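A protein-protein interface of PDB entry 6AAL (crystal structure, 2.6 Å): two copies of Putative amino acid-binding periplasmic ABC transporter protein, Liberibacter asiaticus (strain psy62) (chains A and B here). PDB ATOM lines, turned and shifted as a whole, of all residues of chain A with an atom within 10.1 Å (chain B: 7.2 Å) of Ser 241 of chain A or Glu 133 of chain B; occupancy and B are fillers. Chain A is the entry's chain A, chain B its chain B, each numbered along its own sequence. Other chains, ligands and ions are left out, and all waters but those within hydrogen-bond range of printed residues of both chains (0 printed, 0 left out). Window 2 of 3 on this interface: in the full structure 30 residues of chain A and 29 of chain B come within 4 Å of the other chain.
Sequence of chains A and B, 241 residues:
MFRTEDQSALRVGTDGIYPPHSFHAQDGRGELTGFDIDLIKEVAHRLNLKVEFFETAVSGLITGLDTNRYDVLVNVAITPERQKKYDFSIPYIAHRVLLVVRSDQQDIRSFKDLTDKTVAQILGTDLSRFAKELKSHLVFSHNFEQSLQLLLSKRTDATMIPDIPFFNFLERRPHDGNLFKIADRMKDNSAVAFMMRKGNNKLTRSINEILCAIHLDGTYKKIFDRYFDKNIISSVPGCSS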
ATOM      1  N   GLU A 209     -14.965  34.946 -13.768  1.00  0.00           N
ATOM      2  CA  GLU A 209     -15.107  33.540 -13.389  1.00  0.00           C
ATOM      3  C   GLU A 209     -13.794  32.992 -12.903  1.00  0.00           C
ATOM      4  O   GLU A 209     -13.702  32.313 -11.862  1.00  0.00           O
ATOM      5  CB  GLU A 209     -15.594  32.707 -14.556  1.00  0.00           C
ATOM      6  CG  GLU A 209     -16.230  31.410 -14.107  1.00  0.00           C
ATOM      7  CD  GLU A 209     -16.436  30.416 -15.239  1.00  0.00           C
ATOM      8  OE1 GLU A 209     -16.172  29.203 -14.977  1.00  0.00           O
ATOM      9  OE2 GLU A 209     -16.868  30.852 -16.358  1.00  0.00           O
ATOM     10  N   CYS A 212     -12.735  34.283  -9.605  1.00  0.00           N
ATOM     11  CA  CYS A 212     -13.488  33.559  -8.617  1.00  0.00           C
ATOM     12  C   CYS A 212     -12.809  32.222  -8.250  1.00  0.00           C
ATOM     13  O   CYS A 212     -12.643  31.923  -7.069  1.00  0.00           O
ATOM     14  CB  CYS A 212     -14.896  33.358  -9.130  1.00  0.00           C
ATOM     15  SG  CYS A 212     -15.840  32.430  -7.948  1.00  0.00           S
ATOM     16  N   ALA A 213     -12.392  31.437  -9.257  1.00  0.00           N
ATOM     17  CA  ALA A 213     -11.614  30.185  -9.039  1.00  0.00           C
ATOM     18  C   ALA A 213     -10.267  30.444  -8.387  1.00  0.00           C
ATOM     19  O   ALA A 213      -9.754  29.607  -7.640  1.00  0.00           O
ATOM     20  CB  ALA A 213     -11.410  29.437 -10.350  1.00  0.00           C
ATOM     21  N   HIS A 215      -9.394  32.944  -6.232  1.00  0.00           N
ATOM     22  CA  HIS A 215      -9.787  32.938  -4.811  1.00  0.00           C
ATOM     23  C   HIS A 215     -10.077  31.550  -4.227  1.00  0.00           C
ATOM     24  O   HIS A 215      -9.486  31.154  -3.222  1.00  0.00           O
ATOM     25  CB  HIS A 215     -11.022  33.788  -4.610  1.00  0.00           C
ATOM     26  CG  HIS A 215     -10.726  35.244  -4.492  1.00  0.00           C
ATOM     27  ND1 HIS A 215     -11.006  36.145  -5.497  1.00  0.00           N
ATOM     28  CD2 HIS A 215     -10.170  35.951  -3.483  1.00  0.00           C
ATOM     29  CE1 HIS A 215     -10.635  37.351  -5.106  1.00  0.00           C
ATOM     30  NE2 HIS A 215     -10.130  37.261  -3.886  1.00  0.00           N
ATOM     31  N   LEU A 216     -10.984  30.815  -4.860  1.00  0.00           N
ATOM     32  CA  LEU A 216     -11.403  29.537  -4.294  1.00  0.00           C
ATOM     33  C   LEU A 216     -10.287  28.515  -4.068  1.00  0.00           C
ATOM     34  O   LEU A 216     -10.397  27.762  -3.122  1.00  0.00           O
ATOM     35  CB  LEU A 216     -12.538  28.897  -5.109  1.00  0.00           C
ATOM     36  CG  LEU A 216     -13.911  29.580  -5.004  1.00  0.00           C
ATOM     37  CD1 LEU A 216     -14.895  28.928  -5.954  1.00  0.00           C
ATOM     38  CD2 LEU A 216     -14.441  29.595  -3.569  1.00  0.00           C
ATOM     39  N   ASP A 217      -9.231  28.482  -4.889  1.00  0.00           N
ATOM     40  CA  ASP A 217      -8.156  27.462  -4.712  1.00  0.00           C
ATOM     41  C   ASP A 217      -6.985  27.941  -3.855  1.00  0.00           C
ATOM     42  O   ASP A 217      -6.055  27.181  -3.587  1.00  0.00           O
ATOM     43  CB  ASP A 217      -7.680  26.842  -6.062  1.00  0.00           C
ATOM     44  CG  ASP A 217      -6.738  27.745  -6.873  1.00  0.00           C
ATOM     45  OD1 ASP A 217      -6.527  27.446  -8.048  1.00  0.00           O
ATOM     46  OD2 ASP A 217      -6.179  28.743  -6.373  1.00  0.00           O
ATOM     47  N   GLY A 238     -13.579  37.014  -0.918  1.00  0.00           N
ATOM     48  CA  GLY A 238     -13.383  35.775  -1.677  1.00  0.00           C
ATOM     49  C   GLY A 238     -14.678  35.321  -2.303  1.00  0.00           C
ATOM     50  O   GLY A 238     -15.676  36.032  -2.241  1.00  0.00           O
ATOM     51  N   CYS A 239     -14.669  34.115  -2.873  1.00  0.00           N
ATOM     52  CA  CYS A 239     -15.800  33.579  -3.662  1.00  0.00           C
ATOM     53  C   CYS A 239     -16.555  32.468  -2.939  1.00  0.00           C
ATOM     54  O   CYS A 239     -16.276  32.179  -1.771  1.00  0.00           O
ATOM     55  CB  CYS A 239     -15.280  33.047  -4.994  1.00  0.00           C
ATOM     56  SG  CYS A 239     -16.138  33.731  -6.407  1.00  0.00           S
ATOM     57  N   SER A 240     -17.526  31.871  -3.622  1.00  0.00           N
ATOM     58  CA  SER A 240     -18.220  30.706  -3.095  1.00  0.00           C
ATOM     59  C   SER A 240     -18.217  29.574  -4.111  1.00  0.00           C
ATOM     60  O   SER A 240     -18.471  29.792  -5.302  1.00  0.00           O
ATOM     61  CB  SER A 240     -19.651  31.057  -2.760  1.00  0.00           C
ATOM     62  OG  SER A 240     -19.708  32.109  -1.826  1.00  0.00           O
ATOM     63  N   SER A 241     -17.954  28.366  -3.632  1.00  0.00           N
ATOM     64  CA  SER A 241     -17.941  27.147  -4.473  1.00  0.00           C
ATOM     65  C   SER A 241     -19.157  27.018  -5.368  1.00  0.00           C
ATOM     66  O   SER A 241     -20.273  27.080  -4.886  1.00  0.00           O
ATOM     67  CB  SER A 241     -17.868  25.904  -3.580  1.00  0.00           C
ATOM     68  OG  SER A 241     -16.734  25.964  -2.705  1.00  0.00           O
ATOM     69  N   ILE B  78     -21.596  34.895  -5.187  1.00  0.00           N
ATOM     70  CA  ILE B  78     -20.997  34.638  -6.503  1.00  0.00           C
ATOM     71  C   ILE B  78     -20.321  33.269  -6.450  1.00  0.00           C
ATOM     72  O   ILE B  78     -19.578  32.958  -5.513  1.00  0.00           O
ATOM     73  CB  ILE B  78     -19.962  35.719  -6.918  1.00  0.00           C
ATOM     74  CG1 ILE B  78     -20.464  37.109  -6.517  1.00  0.00           C
ATOM     75  CG2 ILE B  78     -19.661  35.598  -8.394  1.00  0.00           C
ATOM     76  CD1 ILE B  78     -19.878  38.294  -7.272  1.00  0.00           C
ATOM     77  N   THR B  79     -20.637  32.473  -7.454  1.00  0.00           N
ATOM     78  CA  THR B  79     -20.138  31.138  -7.663  1.00  0.00           C
ATOM     79  C   THR B  79     -19.538  31.185  -9.073  1.00  0.00           C
ATOM     80  O   THR B  79     -19.944  32.007  -9.887  1.00  0.00           O
ATOM     81  CB  THR B  79     -21.309  30.122  -7.537  1.00  0.00           C
ATOM     82  OG1 THR B  79     -21.634  29.931  -6.147  1.00  0.00           O
ATOM     83  CG2 THR B  79     -20.991  28.761  -8.145  1.00  0.00           C
ATOM     84  N   PRO B  80     -18.556  30.318  -9.375  1.00  0.00           N
ATOM     85  CA  PRO B  80     -18.075  30.402 -10.746  1.00  0.00           C
ATOM     86  C   PRO B  80     -19.164  30.037 -11.742  1.00  0.00           C
ATOM     87  O   PRO B  80     -19.358  30.776 -12.703  1.00  0.00           O
ATOM     88  CB  PRO B  80     -16.907  29.410 -10.783  1.00  0.00           C
ATOM     89  CG  PRO B  80     -16.484  29.277  -9.359  1.00  0.00           C
ATOM     90  CD  PRO B  80     -17.734  29.419  -8.555  1.00  0.00           C
ATOM     91  N   GLU B  81     -19.866  28.932 -11.509  1.00  0.00           N
ATOM     92  CA  GLU B  81     -20.978  28.525 -12.370  1.00  0.00           C
ATOM     93  C   GLU B  81     -22.130  29.506 -12.440  1.00  0.00           C
ATOM     94  O   GLU B  81     -22.897  29.440 -13.370  1.00  0.00           O
ATOM     95  CB  GLU B  81     -21.570  27.188 -11.939  1.00  0.00           C
ATOM     96  CG  GLU B  81     -20.669  25.999 -12.176  1.00  0.00           C
ATOM     97  CD  GLU B  81     -19.791  25.670 -10.983  1.00  0.00           C
ATOM     98  OE1 GLU B  81     -19.673  26.516 -10.032  1.00  0.00           O
ATOM     99  OE2 GLU B  81     -19.236  24.539 -11.019  1.00  0.00           O
ATOM    100  N   ARG B  82     -22.292  30.392 -11.473  1.00  0.00           N
ATOM    101  CA  ARG B  82     -23.249  31.477 -11.640  1.00  0.00           C
ATOM    102  C   ARG B  82     -22.702  32.567 -12.559  1.00  0.00           C
ATOM    103  O   ARG B  82     -23.440  33.104 -13.402  1.00  0.00           O
ATOM    104  CB  ARG B  82     -23.693  32.068 -10.300  1.00  0.00           C
ATOM    105  CG  ARG B  82     -24.616  31.150  -9.517  1.00  0.00           C
ATOM    106  CD  ARG B  82     -25.307  31.814  -8.331  1.00  0.00           C
ATOM    107  NE  ARG B  82     -25.888  30.784  -7.472  1.00  0.00           N
ATOM    108  CZ  ARG B  82     -25.683  30.662  -6.163  1.00  0.00           C
ATOM    109  NH1 ARG B  82     -24.931  31.542  -5.501  1.00  0.00           N
ATOM    110  NH2 ARG B  82     -26.243  29.652  -5.498  1.00  0.00           N
ATOM    111  N   PHE B 111     -14.505  22.634  10.933  1.00  0.00           N
ATOM    112  CA  PHE B 111     -15.198  22.184   9.728  1.00  0.00           C
ATOM    113  C   PHE B 111     -14.788  20.757   9.293  1.00  0.00           C
ATOM    114  O   PHE B 111     -15.619  19.982   8.798  1.00  0.00           O
ATOM    115  CB  PHE B 111     -14.911  23.143   8.589  1.00  0.00           C
ATOM    116  CG  PHE B 111     -15.572  24.472   8.736  1.00  0.00           C
ATOM    117  CD1 PHE B 111     -16.941  24.563   8.889  1.00  0.00           C
ATOM    118  CD2 PHE B 111     -14.825  25.630   8.682  1.00  0.00           C
ATOM    119  CE1 PHE B 111     -17.550  25.797   9.043  1.00  0.00           C
ATOM    120  CE2 PHE B 111     -15.424  26.864   8.808  1.00  0.00           C
ATOM    121  CZ  PHE B 111     -16.789  26.951   8.989  1.00  0.00           C
ATOM    122  N   ASP B 126     -28.041  29.237   1.626  1.00  0.00           N
ATOM    123  CA  ASP B 126     -27.296  28.810   0.448  1.00  0.00           C
ATOM    124  C   ASP B 126     -25.988  28.135   0.795  1.00  0.00           C
ATOM    125  O   ASP B 126     -24.963  28.483   0.261  1.00  0.00           O
ATOM    126  CB  ASP B 126     -27.015  30.037  -0.392  1.00  0.00           C
ATOM    127  CG  ASP B 126     -26.414  29.715  -1.751  1.00  0.00           C
ATOM    128  OD1 ASP B 126     -26.756  28.687  -2.361  1.00  0.00           O
ATOM    129  OD2 ASP B 126     -25.618  30.553  -2.230  1.00  0.00           O
ATOM    130  N   SER B 128     -25.596  24.467   1.065  1.00  0.00           N
ATOM    131  CA  SER B 128     -25.517  23.091   0.558  1.00  0.00           C
ATOM    132  C   SER B 128     -24.193  22.700  -0.159  1.00  0.00           C
ATOM    133  O   SER B 128     -23.593  21.701   0.183  1.00  0.00           O
ATOM    134  CB  SER B 128     -26.694  22.829  -0.384  1.00  0.00           C
ATOM    135  OG  SER B 128     -27.944  23.216   0.203  1.00  0.00           O
ATOM    136  N   ARG B 129     -23.700  23.475  -1.122  1.00  0.00           N
ATOM    137  CA  ARG B 129     -22.444  23.096  -1.852  1.00  0.00           C
ATOM    138  C   ARG B 129     -21.211  23.123  -0.948  1.00  0.00           C
ATOM    139  O   ARG B 129     -20.422  22.190  -0.966  1.00  0.00           O
ATOM    140  CB  ARG B 129     -22.155  23.999  -3.052  1.00  0.00           C
ATOM    141  CG  ARG B 129     -23.312  24.194  -4.007  1.00  0.00           C
ATOM    142  CD  ARG B 129     -22.953  25.178  -5.094  1.00  0.00           C
ATOM    143  NE  ARG B 129     -22.839  26.531  -4.575  1.00  0.00           N
ATOM    144  CZ  ARG B 129     -23.862  27.325  -4.237  1.00  0.00           C
ATOM    145  NH1 ARG B 129     -25.119  26.910  -4.325  1.00  0.00           N
ATOM    146  NH2 ARG B 129     -23.620  28.553  -3.798  1.00  0.00           N
ATOM    147  N   PHE B 130     -21.039  24.189  -0.160  1.00  0.00           N
ATOM    148  CA  PHE B 130     -19.952  24.235   0.817  1.00  0.00           C
ATOM    149  C   PHE B 130     -19.988  23.061   1.819  1.00  0.00           C
ATOM    150  O   PHE B 130     -18.948  22.627   2.298  1.00  0.00           O
ATOM    151  CB  PHE B 130     -19.950  25.557   1.581  1.00  0.00           C
ATOM    152  CG  PHE B 130     -19.057  25.541   2.791  1.00  0.00           C
ATOM    153  CD1 PHE B 130     -17.681  25.474   2.645  1.00  0.00           C
ATOM    154  CD2 PHE B 130     -19.594  25.544   4.074  1.00  0.00           C
ATOM    155  CE1 PHE B 130     -16.859  25.442   3.748  1.00  0.00           C
ATOM    156  CE2 PHE B 130     -18.772  25.507   5.185  1.00  0.00           C
ATOM    157  CZ  PHE B 130     -17.403  25.464   5.024  1.00  0.00           C
ATOM    158  N   ALA B 131     -21.182  22.554   2.113  1.00  0.00           N
ATOM    159  CA  ALA B 131     -21.392  21.484   3.092  1.00  0.00           C
ATOM    160  C   ALA B 131     -21.236  20.034   2.565  1.00  0.00           C
ATOM    161  O   ALA B 131     -21.194  19.085   3.372  1.00  0.00           O
ATOM    162  CB  ALA B 131     -22.785  21.649   3.691  1.00  0.00           C
ATOM    163  N   LYS B 132     -21.214  19.864   1.236  1.00  0.00           N
ATOM    164  CA  LYS B 132     -21.030  18.554   0.616  1.00  0.00           C
ATOM    165  C   LYS B 132     -19.606  18.087   0.844  1.00  0.00           C
ATOM    166  O   LYS B 132     -19.328  16.887   1.085  1.00  0.00           O
ATOM    167  CB  LYS B 132     -21.262  18.620  -0.902  1.00  0.00           C
ATOM    168  CG  LYS B 132     -20.664  17.429  -1.675  1.00  0.00           C
ATOM    169  CD  LYS B 132     -20.620  17.624  -3.187  1.00  0.00           C
ATOM    170  CE  LYS B 132     -21.898  17.121  -3.853  1.00  0.00           C
ATOM    171  NZ  LYS B 132     -22.071  17.690  -5.218  1.00  0.00           N
ATOM    172  N   GLU B 133     -18.701  19.053   0.747  1.00  0.00           N
ATOM    173  CA  GLU B 133     -17.282  18.756   0.755  1.00  0.00           C
ATOM    174  C   GLU B 133     -16.855  18.225   2.112  1.00  0.00           C
ATOM    175  O   GLU B 133     -15.710  17.824   2.257  1.00  0.00           O
ATOM    176  CB  GLU B 133     -16.472  20.019   0.403  1.00  0.00           C
ATOM    177  CG  GLU B 133     -16.779  20.604  -0.981  1.00  0.00           C
ATOM    178  CD  GLU B 133     -16.518  22.101  -1.100  1.00  0.00           C
ATOM    179  OE1 GLU B 133     -16.491  22.593  -2.248  1.00  0.00           O
ATOM    180  OE2 GLU B 133     -16.350  22.792  -0.063  1.00  0.00           O
ATOM    181  N   LEU B 134     -17.787  18.177   3.074  1.00  0.00           N
ATOM    182  CA  LEU B 134     -17.434  18.373   4.474  1.00  0.00           C
ATOM    183  C   LEU B 134     -17.538  17.253   5.535  1.00  0.00           C
ATOM    184  O   LEU B 134     -17.087  17.478   6.661  1.00  0.00           O
ATOM    185  CB  LEU B 134     -18.147  19.636   4.993  1.00  0.00           C
ATOM    186  CG  LEU B 134     -17.366  20.589   5.923  1.00  0.00           C
ATOM    187  CD1 LEU B 134     -15.949  20.871   5.420  1.00  0.00           C
ATOM    188  CD2 LEU B 134     -18.142  21.901   6.081  1.00  0.00           C
ATOM    189  N   LYS B 135     -18.098  16.078   5.299  1.00  0.00           N
ATOM    190  CA  LYS B 135     -19.077  15.710   4.325  1.00  0.00           C
ATOM    191  C   LYS B 135     -20.165  15.279   5.309  1.00  0.00           C
ATOM    192  O   LYS B 135     -20.249  14.103   5.697  1.00  0.00           O
ATOM    193  CB  LYS B 135     -18.610  14.501   3.499  1.00  0.00           C
ATOM    194  CG  LYS B 135     -17.144  14.484   3.104  1.00  0.00           C
ATOM    195  CD  LYS B 135     -16.294  13.663   4.067  1.00  0.00           C
ATOM    196  CE  LYS B 135     -14.813  13.813   3.733  1.00  0.00           C
ATOM    197  NZ  LYS B 135     -13.904  13.074   4.678  1.00  0.00           N
ATOM    198  N   SER B 136     -20.930  16.261   5.786  1.00  0.00           N
ATOM    199  CA  SER B 136     -21.902  16.043   6.842  1.00  0.00           C
ATOM    200  C   SER B 136     -23.189  15.493   6.250  1.00  0.00           C
ATOM    201  O   SER B 136     -23.413  15.516   5.047  1.00  0.00           O
ATOM    202  CB  SER B 136     -22.191  17.364   7.536  1.00  0.00           C
ATOM    203  OG  SER B 136     -22.438  18.371   6.562  1.00  0.00           O
ATOM    204  N   SER B 190     -16.835  35.373   1.661  1.00  0.00           N
ATOM    205  CA  SER B 190     -17.545  35.125   0.390  1.00  0.00           C
ATOM    206  C   SER B 190     -18.364  36.332  -0.153  1.00  0.00           C
ATOM    207  O   SER B 190     -19.359  36.700   0.450  1.00  0.00           O
ATOM    208  CB  SER B 190     -18.506  33.934   0.584  1.00  0.00           C
ATOM    209  OG  SER B 190     -18.067  32.791  -0.113  1.00  0.00           O
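Among the printed residues, merely in contact across the chains: Glu 209 of chain A with Pro 80 of chain B (3.5 Å), Leu 216 of chain A with Pro 80 of chain B (3.8 Å), Gly 238 of chain A with Ser 190 of chain B (3.4 Å) and Ser 240 of chain A with Pro 80 of chain B (3.4 Å).
The backbone carbonyl oxygen (O) of Cys 239 of chain A is in hydrogen-bond range of the side-chain hydroxyl (OG) of Ser 190 of chain B. N of Ser 240 of chain A is in hydrogen-bond range of O of Ile 78 of chain B (3.0 Å). The backbone carbonyl oxygen (O) of Ser 240 of chain A lies close to the side-chain hydroxyl (OG1) of Thr 79 of chain B. The side-chain hydroxyl (OG) of Ser 190 of chain B lies within hydrogen-bond range of the side-chain hydroxyl (OG) of Ser 240 of chain A, at 2.5 Å. O of Ser 241 of chain A lies within hydrogen-bond range of OG1 of Thr 79 of chain B, 3.4 Å away. O of Ser 241 of chain A is in hydrogen-bond range of NE of Arg 129 of chain B (2.6 Å). OG of Ser 241 of chain A lies within hydrogen-bond range of OE1 of Glu 133 of chain B (3.4 Å). The side-chain sulfur (SG) of Cys 212 of chain A lies close to the backbone nitrogen (N) of Pro 80 of chain B (3.7 Å). The side-chain sulfur (SG) of Cys 239 of chain A lies close to the backbone carbonyl oxygen (O) of Ile 78 of chain B (3.6 Å).
Ser 241 of chain A touches just these residues of chain B: Thr 79, Arg 129 and Glu 133. Glu 133 of chain B touches just one residue of chain A: Ser 241 (3.4 Å). No residue of chain A comes within 4 Å of Leu 134 of chain B. Printed residues of chain B within 4 Å of Leu 216 of chain A: Pro 80. Of the printed residues of chain A, Ser 190 of chain B touches Gly 238 (3.4 Å), Cys 239 (2.5 Å) and Ser 240 (2.5 Å). Of the printed residues of chain A, Ile 78 of chain B touches Cys 239 and Ser 240. Of the printed residues of chain B, Cys 212 of chain A touches Pro 80. Of the printed residues of chain B, Cys 239 of chain A touches Ile 78 (3.6 Å) and Ser 190 (2.5 Å). Arg 82 of chain B touches none of the printed residues of chain A. Phe 111 of chain B touches none of the printed residues of chain A. The nearest printed residue of chain A that does not touch Glu 133 of chain B is Leu 216 of chain A (7.4 Å). The nearest printed residue of chain A that does not touch Ile 78 of chain B is Cys 212 of chain A (4.5 Å).
Of the 17 printed residues of chain B, 6 touch a printed residue of chain A. Hydrophobic or aromatic side chains of chain B within 4 Å of the printed part of chain A: Pro 80. Among the printed residues, 13 pairs touch across the chains. Among the printed residues, no Asp or Glu carboxylate lies within 4 Å of a Lys or Arg side-chain nitrogen of the other chain.
No position is printed for both chains. Of the 13 pairs that touch across the chains among the printed residues, none has its exchanged pair printed and touching as well.
The side-chain sulfur (SG) of Cys 212 of chain A is disulfide-bonded to the side-chain sulfur (SG) of Cys 239 of chain A. The side-chain hydroxyl (OG1) of Thr 79 of chain B lies within hydrogen-bond range of the guanidinium group (NH2) of Arg 129 of chain B. The side-chain carboxylate of Asp 126 of chain B is in salt-bridge range of the guanidinium group of Arg 129 of chain B.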
